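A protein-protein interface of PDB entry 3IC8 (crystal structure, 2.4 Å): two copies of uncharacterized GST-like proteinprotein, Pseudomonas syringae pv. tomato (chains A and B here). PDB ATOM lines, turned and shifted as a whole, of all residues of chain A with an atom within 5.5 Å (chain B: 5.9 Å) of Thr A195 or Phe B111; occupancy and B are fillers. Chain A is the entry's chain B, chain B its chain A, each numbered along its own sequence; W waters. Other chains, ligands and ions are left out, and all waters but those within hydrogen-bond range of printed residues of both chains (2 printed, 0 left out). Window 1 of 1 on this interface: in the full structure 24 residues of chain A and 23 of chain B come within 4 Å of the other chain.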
ATOM      1  N   VAL A 110      -9.781 -16.483  31.982  1.00  0.00           N
ATOM      2  CA  VAL A 110     -10.313 -16.425  30.650  1.00  0.00           C
ATOM      3  C   VAL A 110     -10.052 -15.157  29.864  1.00  0.00           C
ATOM      4  O   VAL A 110      -9.617 -15.206  28.758  1.00  0.00           O
ATOM      5  CB  VAL A 110     -11.822 -16.568  30.730  1.00  0.00           C
ATOM      6  CG1 VAL A 110     -12.452 -16.279  29.433  1.00  0.00           C
ATOM      7  CG2 VAL A 110     -12.183 -17.899  31.185  1.00  0.00           C
ATOM      8  N   PHE A 111     -10.348 -14.010  30.423  1.00  0.00           N
ATOM      9  CA  PHE A 111     -10.309 -12.821  29.626  1.00  0.00           C
ATOM     10  C   PHE A 111      -8.945 -12.213  29.574  1.00  0.00           C
ATOM     11  O   PHE A 111      -8.699 -11.196  30.130  1.00  0.00           O
ATOM     12  CB  PHE A 111     -11.355 -11.828  30.083  1.00  0.00           C
ATOM     13  CG  PHE A 111     -12.744 -12.320  29.912  1.00  0.00           C
ATOM     14  CD1 PHE A 111     -13.322 -12.400  28.674  1.00  0.00           C
ATOM     15  CD2 PHE A 111     -13.471 -12.724  30.987  1.00  0.00           C
ATOM     16  CE1 PHE A 111     -14.583 -12.869  28.537  1.00  0.00           C
ATOM     17  CE2 PHE A 111     -14.716 -13.188  30.838  1.00  0.00           C
ATOM     18  CZ  PHE A 111     -15.276 -13.261  29.619  1.00  0.00           C
ATOM     19  N   GLN A 112      -8.058 -12.877  28.870  1.00  0.00           N
ATOM     20  CA  GLN A 112      -6.738 -12.378  28.648  1.00  0.00           C
ATOM     21  C   GLN A 112      -6.265 -12.901  27.316  1.00  0.00           C
ATOM     22  O   GLN A 112      -6.788 -13.841  26.814  1.00  0.00           O
ATOM     23  CB  GLN A 112      -5.816 -12.733  29.808  1.00  0.00           C
ATOM     24  CG  GLN A 112      -5.852 -14.133  30.259  1.00  0.00           C
ATOM     25  CD  GLN A 112      -4.536 -14.555  30.820  1.00  0.00           C
ATOM     26  OE1 GLN A 112      -3.574 -13.839  30.714  1.00  0.00           O
ATOM     27  NE2 GLN A 112      -4.484 -15.715  31.424  1.00  0.00           N
ATOM     28  N   PRO A 113      -5.248 -12.295  26.759  1.00  0.00           N
ATOM     29  CA  PRO A 113      -4.881 -12.500  25.372  1.00  0.00           C
ATOM     30  C   PRO A 113      -4.471 -13.911  25.017  1.00  0.00           C
ATOM     31  O   PRO A 113      -4.605 -14.320  23.888  1.00  0.00           O
ATOM     32  CB  PRO A 113      -3.735 -11.527  25.204  1.00  0.00           C
ATOM     33  CG  PRO A 113      -4.131 -10.437  25.991  1.00  0.00           C
ATOM     34  CD  PRO A 113      -4.810 -10.977  27.199  1.00  0.00           C
ATOM     35  N   SER A 115      -5.888 -16.516  25.520  1.00  0.00           N
ATOM     36  CA  SER A 115      -7.043 -17.325  25.208  1.00  0.00           C
ATOM     37  C   SER A 115      -7.486 -17.192  23.773  1.00  0.00           C
ATOM     38  O   SER A 115      -8.459 -17.776  23.386  1.00  0.00           O
ATOM     39  CB  SER A 115      -8.215 -16.966  26.112  1.00  0.00           C
ATOM     40  OG  SER A 115      -8.001 -17.375  27.427  1.00  0.00           O
ATOM     41  N   MET A 116      -6.762 -16.429  22.983  1.00  0.00           N
ATOM     42  CA  MET A 116      -7.149 -16.168  21.614  1.00  0.00           C
ATOM     43  C   MET A 116      -6.930 -17.333  20.669  1.00  0.00           C
ATOM     44  O   MET A 116      -6.114 -18.197  20.917  1.00  0.00           O
ATOM     45  CB  MET A 116      -6.396 -14.964  21.090  1.00  0.00           C
ATOM     46  CG  MET A 116      -6.991 -13.672  21.463  1.00  0.00           C
ATOM     47  SD  MET A 116      -5.820 -12.303  20.920  1.00  0.00           S
ATOM     48  CE  MET A 116      -6.082 -11.009  22.282  1.00  0.00           C
ATOM     49  N   PHE A 191     -17.057 -20.380  32.536  1.00  0.00           N
ATOM     50  CA  PHE A 191     -16.200 -19.514  31.787  1.00  0.00           C
ATOM     51  C   PHE A 191     -15.009 -20.236  31.221  1.00  0.00           C
ATOM     52  O   PHE A 191     -14.643 -20.003  30.136  1.00  0.00           O
ATOM     53  CB  PHE A 191     -15.715 -18.376  32.660  1.00  0.00           C
ATOM     54  CG  PHE A 191     -16.746 -17.370  32.959  1.00  0.00           C
ATOM     55  CD1 PHE A 191     -16.792 -16.199  32.278  1.00  0.00           C
ATOM     56  CD2 PHE A 191     -17.648 -17.582  33.932  1.00  0.00           C
ATOM     57  CE1 PHE A 191     -17.733 -15.292  32.553  1.00  0.00           C
ATOM     58  CE2 PHE A 191     -18.579 -16.680  34.199  1.00  0.00           C
ATOM     59  CZ  PHE A 191     -18.623 -15.533  33.513  1.00  0.00           C
ATOM     60  N   LEU A 192     -14.382 -21.090  31.990  1.00  0.00           N
ATOM     61  CA  LEU A 192     -13.183 -21.785  31.571  1.00  0.00           C
ATOM     62  C   LEU A 192     -13.383 -22.744  30.401  1.00  0.00           C
ATOM     63  O   LEU A 192     -12.521 -22.913  29.583  1.00  0.00           O
ATOM     64  CB  LEU A 192     -12.567 -22.490  32.750  1.00  0.00           C
ATOM     65  CG  LEU A 192     -11.710 -21.780  33.775  1.00  0.00           C
ATOM     66  CD1 LEU A 192     -11.297 -20.446  33.410  1.00  0.00           C
ATOM     67  CD2 LEU A 192     -12.409 -21.752  35.031  1.00  0.00           C
ATOM     68  N   LYS A 193     -14.561 -23.344  30.371  1.00  0.00           N
ATOM     69  CA  LYS A 193     -15.004 -24.312  29.397  1.00  0.00           C
ATOM     70  C   LYS A 193     -15.239 -23.738  28.015  1.00  0.00           C
ATOM     71  O   LYS A 193     -15.340 -24.449  27.063  1.00  0.00           O
ATOM     72  CB  LYS A 193     -16.253 -25.002  29.907  1.00  0.00           C
ATOM     73  CG  LYS A 193     -15.992 -25.951  31.013  1.00  0.00           C
ATOM     74  CD  LYS A 193     -16.567 -27.282  30.729  1.00  0.00           C
ATOM     75  CE  LYS A 193     -15.498 -28.262  30.441  1.00  0.00           C
ATOM     76  NZ  LYS A 193     -15.929 -29.636  30.646  1.00  0.00           N
ATOM     77  N   GLN A 194     -15.332 -22.428  27.942  1.00  0.00           N
ATOM     78  CA  GLN A 194     -15.530 -21.693  26.712  1.00  0.00           C
ATOM     79  C   GLN A 194     -14.435 -21.715  25.655  1.00  0.00           C
ATOM     80  O   GLN A 194     -14.724 -21.603  24.497  1.00  0.00           O
ATOM     81  CB  GLN A 194     -15.983 -20.281  26.992  1.00  0.00           C
ATOM     82  CG  GLN A 194     -17.098 -20.205  27.961  1.00  0.00           C
ATOM     83  CD  GLN A 194     -18.360 -20.729  27.421  1.00  0.00           C
ATOM     84  OE1 GLN A 194     -18.822 -20.273  26.427  1.00  0.00           O
ATOM     85  NE2 GLN A 194     -18.918 -21.692  28.070  1.00  0.00           N
ATOM     86  N   THR A 195     -13.182 -21.821  26.061  1.00  0.00           N
ATOM     87  CA  THR A 195     -12.072 -21.814  25.124  1.00  0.00           C
ATOM     88  C   THR A 195     -11.129 -22.986  25.333  1.00  0.00           C
ATOM     89  O   THR A 195     -11.054 -23.523  26.394  1.00  0.00           O
ATOM     90  CB  THR A 195     -11.289 -20.512  25.153  1.00  0.00           C
ATOM     91  OG1 THR A 195     -10.379 -20.533  26.231  1.00  0.00           O
ATOM     92  CG2 THR A 195     -12.177 -19.379  25.326  1.00  0.00           C
ATOM     93  N   PRO A 196     -10.426 -23.384  24.289  1.00  0.00           N
ATOM     94  CA  PRO A 196      -9.526 -24.514  24.339  1.00  0.00           C
ATOM     95  C   PRO A 196      -8.405 -24.296  25.310  1.00  0.00           C
ATOM     96  O   PRO A 196      -8.017 -25.174  26.028  1.00  0.00           O
ATOM     97  CB  PRO A 196      -8.982 -24.543  22.926  1.00  0.00           C
ATOM     98  CG  PRO A 196     -10.039 -24.091  22.147  1.00  0.00           C
ATOM     99  CD  PRO A 196     -10.819 -23.119  22.912  1.00  0.00           C
ATOM    100  N   VAL A 197      -7.902 -23.091  25.318  1.00  0.00           N
ATOM    101  CA  VAL A 197      -6.875 -22.708  26.231  1.00  0.00           C
ATOM    102  C   VAL A 197      -7.267 -22.749  27.691  1.00  0.00           C
ATOM    103  O   VAL A 197      -6.485 -23.131  28.494  1.00  0.00           O
ATOM    104  CB  VAL A 197      -6.355 -21.354  25.857  1.00  0.00           C
ATOM    105  CG1 VAL A 197      -5.598 -20.762  26.950  1.00  0.00           C
ATOM    106  CG2 VAL A 197      -5.519 -21.464  24.655  1.00  0.00           C
ATOM    107  N   THR A 198      -8.470 -22.350  28.047  1.00  0.00           N
ATOM    108  CA  THR A 198      -8.841 -22.333  29.452  1.00  0.00           C
ATOM    109  C   THR A 198      -9.468 -23.611  29.979  1.00  0.00           C
ATOM    110  O   THR A 198      -9.546 -23.811  31.146  1.00  0.00           O
ATOM    111  CB  THR A 198      -9.692 -21.088  29.820  1.00  0.00           C
ATOM    112  OG1 THR A 198     -10.917 -21.093  29.105  1.00  0.00           O
ATOM    113  CG2 THR A 198      -8.969 -19.853  29.495  1.00  0.00           C
ATOM    114  N   ALA A 199      -9.865 -24.501  29.101  1.00  0.00           N
ATOM    115  CA  ALA A 199     -10.610 -25.689  29.487  1.00  0.00           C
ATOM    116  C   ALA A 199      -9.912 -26.685  30.415  1.00  0.00           C
ATOM    117  O   ALA A 199     -10.545 -27.357  31.176  1.00  0.00           O
ATOM    118  CB  ALA A 199     -11.149 -26.368  28.307  1.00  0.00           C
ATOM    119  N   PRO A 200      -8.605 -26.759  30.325  1.00  0.00           N
ATOM    120  CA  PRO A 200      -7.804 -27.612  31.177  1.00  0.00           C
ATOM    121  C   PRO A 200      -7.861 -27.196  32.619  1.00  0.00           C
ATOM    122  O   PRO A 200      -7.676 -28.012  33.473  1.00  0.00           O
ATOM    123  CB  PRO A 200      -6.425 -27.444  30.603  1.00  0.00           C
ATOM    124  CG  PRO A 200      -6.676 -27.213  29.221  1.00  0.00           C
ATOM    125  CD  PRO A 200      -7.852 -26.353  29.145  1.00  0.00           C
ATOM    126  N   TYR B   9     -15.132 -29.885  20.809  1.00  0.00           N
ATOM    127  CA  TYR B   9     -15.320 -29.611  22.192  1.00  0.00           C
ATOM    128  C   TYR B   9     -16.554 -28.782  22.249  1.00  0.00           C
ATOM    129  O   TYR B   9     -16.598 -27.702  21.762  1.00  0.00           O
ATOM    130  CB  TYR B   9     -14.117 -28.872  22.736  1.00  0.00           C
ATOM    131  CG  TYR B   9     -14.037 -28.807  24.227  1.00  0.00           C
ATOM    132  CD1 TYR B   9     -13.677 -29.896  24.977  1.00  0.00           C
ATOM    133  CD2 TYR B   9     -14.316 -27.648  24.883  1.00  0.00           C
ATOM    134  CE1 TYR B   9     -13.617 -29.822  26.308  1.00  0.00           C
ATOM    135  CE2 TYR B   9     -14.254 -27.575  26.206  1.00  0.00           C
ATOM    136  CZ  TYR B   9     -13.907 -28.655  26.916  1.00  0.00           C
ATOM    137  OH  TYR B   9     -13.854 -28.543  28.243  1.00  0.00           O
ATOM    138  N   THR B  11     -18.426 -27.049  24.386  1.00  0.00           N
ATOM    139  CA  THR B  11     -18.609 -25.753  24.966  1.00  0.00           C
ATOM    140  C   THR B  11     -17.679 -24.707  24.394  1.00  0.00           C
ATOM    141  O   THR B  11     -17.696 -23.595  24.817  1.00  0.00           O
ATOM    142  CB  THR B  11     -18.470 -25.802  26.468  1.00  0.00           C
ATOM    143  OG1 THR B  11     -17.280 -26.484  26.809  1.00  0.00           O
ATOM    144  CG2 THR B  11     -19.601 -26.527  27.050  1.00  0.00           C
ATOM    145  N   SER B  12     -16.874 -25.080  23.426  1.00  0.00           N
ATOM    146  CA  SER B  12     -15.933 -24.155  22.852  1.00  0.00           C
ATOM    147  C   SER B  12     -16.581 -23.222  21.861  1.00  0.00           C
ATOM    148  O   SER B  12     -17.229 -23.623  20.951  1.00  0.00           O
ATOM    149  CB  SER B  12     -14.791 -24.908  22.207  1.00  0.00           C
ATOM    150  OG  SER B  12     -13.941 -24.044  21.521  1.00  0.00           O
ATOM    151  N   LEU B  13     -16.366 -21.947  22.073  1.00  0.00           N
ATOM    152  CA  LEU B  13     -16.804 -20.889  21.205  1.00  0.00           C
ATOM    153  C   LEU B  13     -16.154 -21.023  19.875  1.00  0.00           C
ATOM    154  O   LEU B  13     -16.693 -20.644  18.890  1.00  0.00           O
ATOM    155  CB  LEU B  13     -16.444 -19.551  21.791  1.00  0.00           C
ATOM    156  CG  LEU B  13     -17.062 -19.147  23.107  1.00  0.00           C
ATOM    157  CD1 LEU B  13     -16.282 -18.041  23.652  1.00  0.00           C
ATOM    158  CD2 LEU B  13     -18.440 -18.708  22.881  1.00  0.00           C
ATOM    159  N   PHE B  14     -14.961 -21.561  19.879  1.00  0.00           N
ATOM    160  CA  PHE B  14     -14.184 -21.760  18.687  1.00  0.00           C
ATOM    161  C   PHE B  14     -14.757 -22.784  17.727  1.00  0.00           C
ATOM    162  O   PHE B  14     -14.502 -22.734  16.558  1.00  0.00           O
ATOM    163  CB  PHE B  14     -12.731 -22.022  19.030  1.00  0.00           C
ATOM    164  CG  PHE B  14     -12.019 -20.830  19.575  1.00  0.00           C
ATOM    165  CD1 PHE B  14     -11.310 -20.006  18.771  1.00  0.00           C
ATOM    166  CD2 PHE B  14     -12.075 -20.535  20.901  1.00  0.00           C
ATOM    167  CE1 PHE B  14     -10.694 -18.941  19.277  1.00  0.00           C
ATOM    168  CE2 PHE B  14     -11.453 -19.469  21.390  1.00  0.00           C
ATOM    169  CZ  PHE B  14     -10.765 -18.678  20.589  1.00  0.00           C
ATOM    170  N   ALA B 106     -12.165  -9.721  16.303  1.00  0.00           N
ATOM    171  CA  ALA B 106     -13.192 -10.069  17.253  1.00  0.00           C
ATOM    172  C   ALA B 106     -12.657 -10.711  18.518  1.00  0.00           C
ATOM    173  O   ALA B 106     -13.089 -10.402  19.576  1.00  0.00           O
ATOM    174  CB  ALA B 106     -14.219 -10.930  16.608  1.00  0.00           C
ATOM    175  N   VAL B 107     -11.722 -11.619  18.378  1.00  0.00           N
ATOM    176  CA  VAL B 107     -11.051 -12.235  19.504  1.00  0.00           C
ATOM    177  C   VAL B 107     -10.151 -11.349  20.346  1.00  0.00           C
ATOM    178  O   VAL B 107     -10.004 -11.581  21.507  1.00  0.00           O
ATOM    179  CB  VAL B 107     -10.438 -13.582  19.169  1.00  0.00           C
ATOM    180  CG1 VAL B 107     -11.475 -14.470  18.654  1.00  0.00           C
ATOM    181  CG2 VAL B 107      -9.369 -13.452  18.194  1.00  0.00           C
ATOM    182  N   SER B 108      -9.508 -10.383  19.729  1.00  0.00           N
ATOM    183  CA  SER B 108      -8.723  -9.424  20.460  1.00  0.00           C
ATOM    184  C   SER B 108      -9.576  -8.591  21.364  1.00  0.00           C
ATOM    185  O   SER B 108      -9.192  -8.283  22.455  1.00  0.00           O
ATOM    186  CB  SER B 108      -7.969  -8.486  19.527  1.00  0.00           C
ATOM    187  OG  SER B 108      -7.023  -9.155  18.764  1.00  0.00           O
ATOM    188  N   LEU B 109     -10.718  -8.185  20.868  1.00  0.00           N
ATOM    189  CA  LEU B 109     -11.603  -7.372  21.619  1.00  0.00           C
ATOM    190  C   LEU B 109     -12.162  -8.043  22.828  1.00  0.00           C
ATOM    191  O   LEU B 109     -12.249  -7.452  23.856  1.00  0.00           O
ATOM    192  CB  LEU B 109     -12.761  -6.973  20.743  1.00  0.00           C
ATOM    193  CG  LEU B 109     -12.562  -5.859  19.751  1.00  0.00           C
ATOM    194  CD1 LEU B 109     -13.782  -5.659  18.952  1.00  0.00           C
ATOM    195  CD2 LEU B 109     -12.215  -4.636  20.453  1.00  0.00           C
ATOM    196  N   VAL B 110     -12.616  -9.258  22.669  1.00  0.00           N
ATOM    197  CA  VAL B 110     -13.171 -10.017  23.745  1.00  0.00           C
ATOM    198  C   VAL B 110     -12.211 -10.478  24.814  1.00  0.00           C
ATOM    199  O   VAL B 110     -12.473 -10.351  25.989  1.00  0.00           O
ATOM    200  CB  VAL B 110     -13.847 -11.231  23.178  1.00  0.00           C
ATOM    201  CG1 VAL B 110     -14.350 -12.107  24.247  1.00  0.00           C
ATOM    202  CG2 VAL B 110     -14.931 -10.827  22.277  1.00  0.00           C
ATOM    203  N   PHE B 111     -11.108 -11.058  24.402  1.00  0.00           N
ATOM    204  CA  PHE B 111     -10.210 -11.663  25.342  1.00  0.00           C
ATOM    205  C   PHE B 111      -9.179 -10.699  25.871  1.00  0.00           C
ATOM    206  O   PHE B 111      -8.023 -10.872  25.687  1.00  0.00           O
ATOM    207  CB  PHE B 111      -9.588 -12.900  24.730  1.00  0.00           C
ATOM    208  CG  PHE B 111     -10.569 -13.961  24.427  1.00  0.00           C
ATOM    209  CD1 PHE B 111     -11.212 -14.611  25.428  1.00  0.00           C
ATOM    210  CD2 PHE B 111     -10.871 -14.299  23.146  1.00  0.00           C
ATOM    211  CE1 PHE B 111     -12.110 -15.563  25.144  1.00  0.00           C
ATOM    212  CE2 PHE B 111     -11.758 -15.256  22.883  1.00  0.00           C
ATOM    213  CZ  PHE B 111     -12.381 -15.880  23.875  1.00  0.00           C
ATOM    214  N   GLN B 112      -9.651  -9.668  26.531  1.00  0.00           N
ATOM    215  CA  GLN B 112      -8.820  -8.726  27.211  1.00  0.00           C
ATOM    216  C   GLN B 112      -9.518  -8.412  28.510  1.00  0.00           C
ATOM    217  O   GLN B 112     -10.678  -8.631  28.638  1.00  0.00           O
ATOM    218  CB  GLN B 112      -8.564  -7.485  26.369  1.00  0.00           C
ATOM    219  CG  GLN B 112      -9.764  -6.878  25.798  1.00  0.00           C
ATOM    220  CD  GLN B 112      -9.517  -5.496  25.260  1.00  0.00           C
ATOM    221  OE1 GLN B 112      -8.893  -4.667  25.901  1.00  0.00           O
ATOM    222  NE2 GLN B 112     -10.026  -5.233  24.085  1.00  0.00           N
ATOM    223  N   PRO B 113      -8.787  -7.887  29.464  1.00  0.00           N
ATOM    224  CA  PRO B 113      -9.208  -7.746  30.844  1.00  0.00           C
ATOM    225  C   PRO B 113     -10.391  -6.843  30.991  1.00  0.00           C
ATOM    226  O   PRO B 113     -11.142  -6.953  31.915  1.00  0.00           O
ATOM    227  CB  PRO B 113      -8.010  -7.091  31.474  1.00  0.00           C
ATOM    228  CG  PRO B 113      -6.912  -7.542  30.719  1.00  0.00           C
ATOM    229  CD  PRO B 113      -7.336  -7.869  29.355  1.00  0.00           C
ATOM    230  N   SER B 115     -13.044  -6.855  29.598  1.00  0.00           N
ATOM    231  CA  SER B 115     -14.316  -7.539  29.423  1.00  0.00           C
ATOM    232  C   SER B 115     -14.875  -8.190  30.660  1.00  0.00           C
ATOM    233  O   SER B 115     -15.970  -8.692  30.618  1.00  0.00           O
ATOM    234  CB  SER B 115     -14.221  -8.608  28.331  1.00  0.00           C
ATOM    235  OG  SER B 115     -13.628  -8.118  27.166  1.00  0.00           O
ATOM    236  N   PHE B 191     -18.493 -14.245  19.244  1.00  0.00           N
ATOM    237  CA  PHE B 191     -17.583 -13.975  20.330  1.00  0.00           C
ATOM    238  C   PHE B 191     -17.956 -12.695  21.059  1.00  0.00           C
ATOM    239  O   PHE B 191     -17.943 -12.656  22.250  1.00  0.00           O
ATOM    240  CB  PHE B 191     -16.139 -13.892  19.828  1.00  0.00           C
ATOM    241  CG  PHE B 191     -15.521 -15.209  19.520  1.00  0.00           C
ATOM    242  CD1 PHE B 191     -14.838 -15.904  20.470  1.00  0.00           C
ATOM    243  CD2 PHE B 191     -15.611 -15.748  18.278  1.00  0.00           C
ATOM    244  CE1 PHE B 191     -14.275 -17.100  20.178  1.00  0.00           C
ATOM    245  CE2 PHE B 191     -15.068 -16.940  17.997  1.00  0.00           C
ATOM    246  CZ  PHE B 191     -14.398 -17.618  18.942  1.00  0.00           C
HETATM  247  O   HOH W   1     -15.803 -31.314  28.109  1.00  0.00           O
HETATM  248  O   HOH W   2     -19.822 -22.224  24.235  1.00  0.00           O
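The side-chain hydroxyl of Tyr B9 sits close to the side-chain amino group of Lys A193. The side-chain hydroxyl (OG1) of Thr B11 sits at hydrogen-bond distance from the backbone carbonyl oxygen (O) of Lys A193, 2.8 Å away. The backbone NH of Leu B13 lies within hydrogen-bond range of the backbone carbonyl oxygen of Gln A194 (2.9 Å). N of Pro B113 sits close to O of Phe A111, at 3.4 Å. The backbone carbonyl oxygen (O) of Gln A112 sits close to the backbone carbonyl oxygen (O) of Phe B111, 3.4 Å away. The backbone carbonyl oxygen of Phe B111 lies close to the backbone nitrogen of Pro A113 (3.3 Å).
The side-chain hydroxyl (OG) of Ser B12 lies close to the backbone NH (N) of Phe B14 (3.1 Å). O of Leu B109 sits at hydrogen-bond distance from NE2 of Gln B112 (3.1 Å). O of Gln B112 lies within hydrogen-bond range of OG of Ser B115, at 3.3 Å. The side-chain hydroxyl (OG) of Ser A115 is in hydrogen-bond range of the backbone carbonyl oxygen (O) of Val A110 (3.0 Å). O of Leu A192 is in hydrogen-bond range of N of Ala A199, 3.1 Å away. The side-chain hydroxyl of Thr A198 sits at hydrogen-bond distance from the side-chain hydroxyl of Thr A195, at 3.0 Å.
Among the printed residues, pairs that only touch across the chains: Val A110 with Phe B111, Phe A111 with Val B110, Phe A111 with Gln B112, Phe A111 with Ser B115, Ser A115 with Phe B14, Ser A115 with Phe B111, Met A116 with Val B107, Met A116 with Ser B108, Met A116 with Phe B111, Lys A193 with Ser B12, Gln A194 with Thr B11, Gln A194 with Ser B12, Thr A195 with Phe B14, Thr A195 with Phe B111, Pro A196 with Ser B12, Pro A196 with Phe B14 and Ala A199 with Tyr B9.
Printed residues of chain B within 4 Å of Ser A115: Phe B14 and Phe B111. Printed residues of chain B within 4 Å of Met A116: Val B107, Ser B108 and Phe B111. Phe A191 touches none of the printed residues of chain B. Of chain B, only Phe B14 (3.9 Å) and Phe B111 (3.8 Å) come within 4 Å of Thr A195. Of the printed residues of chain B, Pro A196 touches Ser B12 and Phe B14. Of the printed residues of chain A, Ser B12 touches Lys A193 (3.997 Å), Gln A194 (3.3 Å) and Pro A196 (3.5 Å). Printed residues of chain A within 4 Å of Phe B14: Ser A115, Thr A195 and Pro A196. Leu B109 touches none of the printed residues of chain A. Of the printed residues of chain A, Phe B111 touches Val A110 (3.7 Å), Gln A112 (3.1 Å), Pro A113 (3.3 Å), Ser A115 (3.9 Å), Met A116 (3.9 Å) and Thr A195 (3.8 Å). The nearest printed residue of chain B that does not touch Thr A195 is Leu B13 (4.6 Å). The nearest printed residue of chain A that does not touch Phe B111 is Phe A111 (4.01 Å).
Printed residues of chain A that touch a printed residue of chain B: Val A110, Phe A111, Gln A112, Pro A113, Ser A115, Met A116, Lys A193, Gln A194, Thr A195, Pro A196 and Ala A199. Of the 15 printed residues of chain B, 12 touch a printed residue of chain A. Printed residues of chain B that touch a printed residue of chain A: Tyr B9, Thr B11, Ser B12, Leu B13, Phe B14, Val B107, Ser B108, Val B110, Phe B111, Gln B112, Pro B113 and Ser B115. Hydrophobic or aromatic side chains of chain B within 4 Å of the printed part of chain A: Tyr B9, Leu B13, Phe B14, Phe B111 and Pro B113.
Val A110 touches Phe B111, and with the chains exchanged Phe A111 touches Val B110. Phe A111 touches Gln B112, and with the chains exchanged Gln A112 touches Phe B111. Phe A111 touches Pro B113, and with the chains exchanged Pro A113 touches Phe B111. Phe A111 touches Ser B115, and with the chains exchanged Ser A115 touches Phe B111. Positions printed for both chains: 110, 111, 112, 113, 115 and 191. Of the 23 pairs that touch across the chains among the printed residues, 8 have their exchanged pair printed and touching as well.
Water W2 lies within hydrogen-bond range of O of Thr B11 and OE1 of Gln A194. Water W1 bridges the side-chain amino group of Lys A193 (3.0 Å) and the side-chain hydroxyl of Tyr B9 (3.4 Å).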
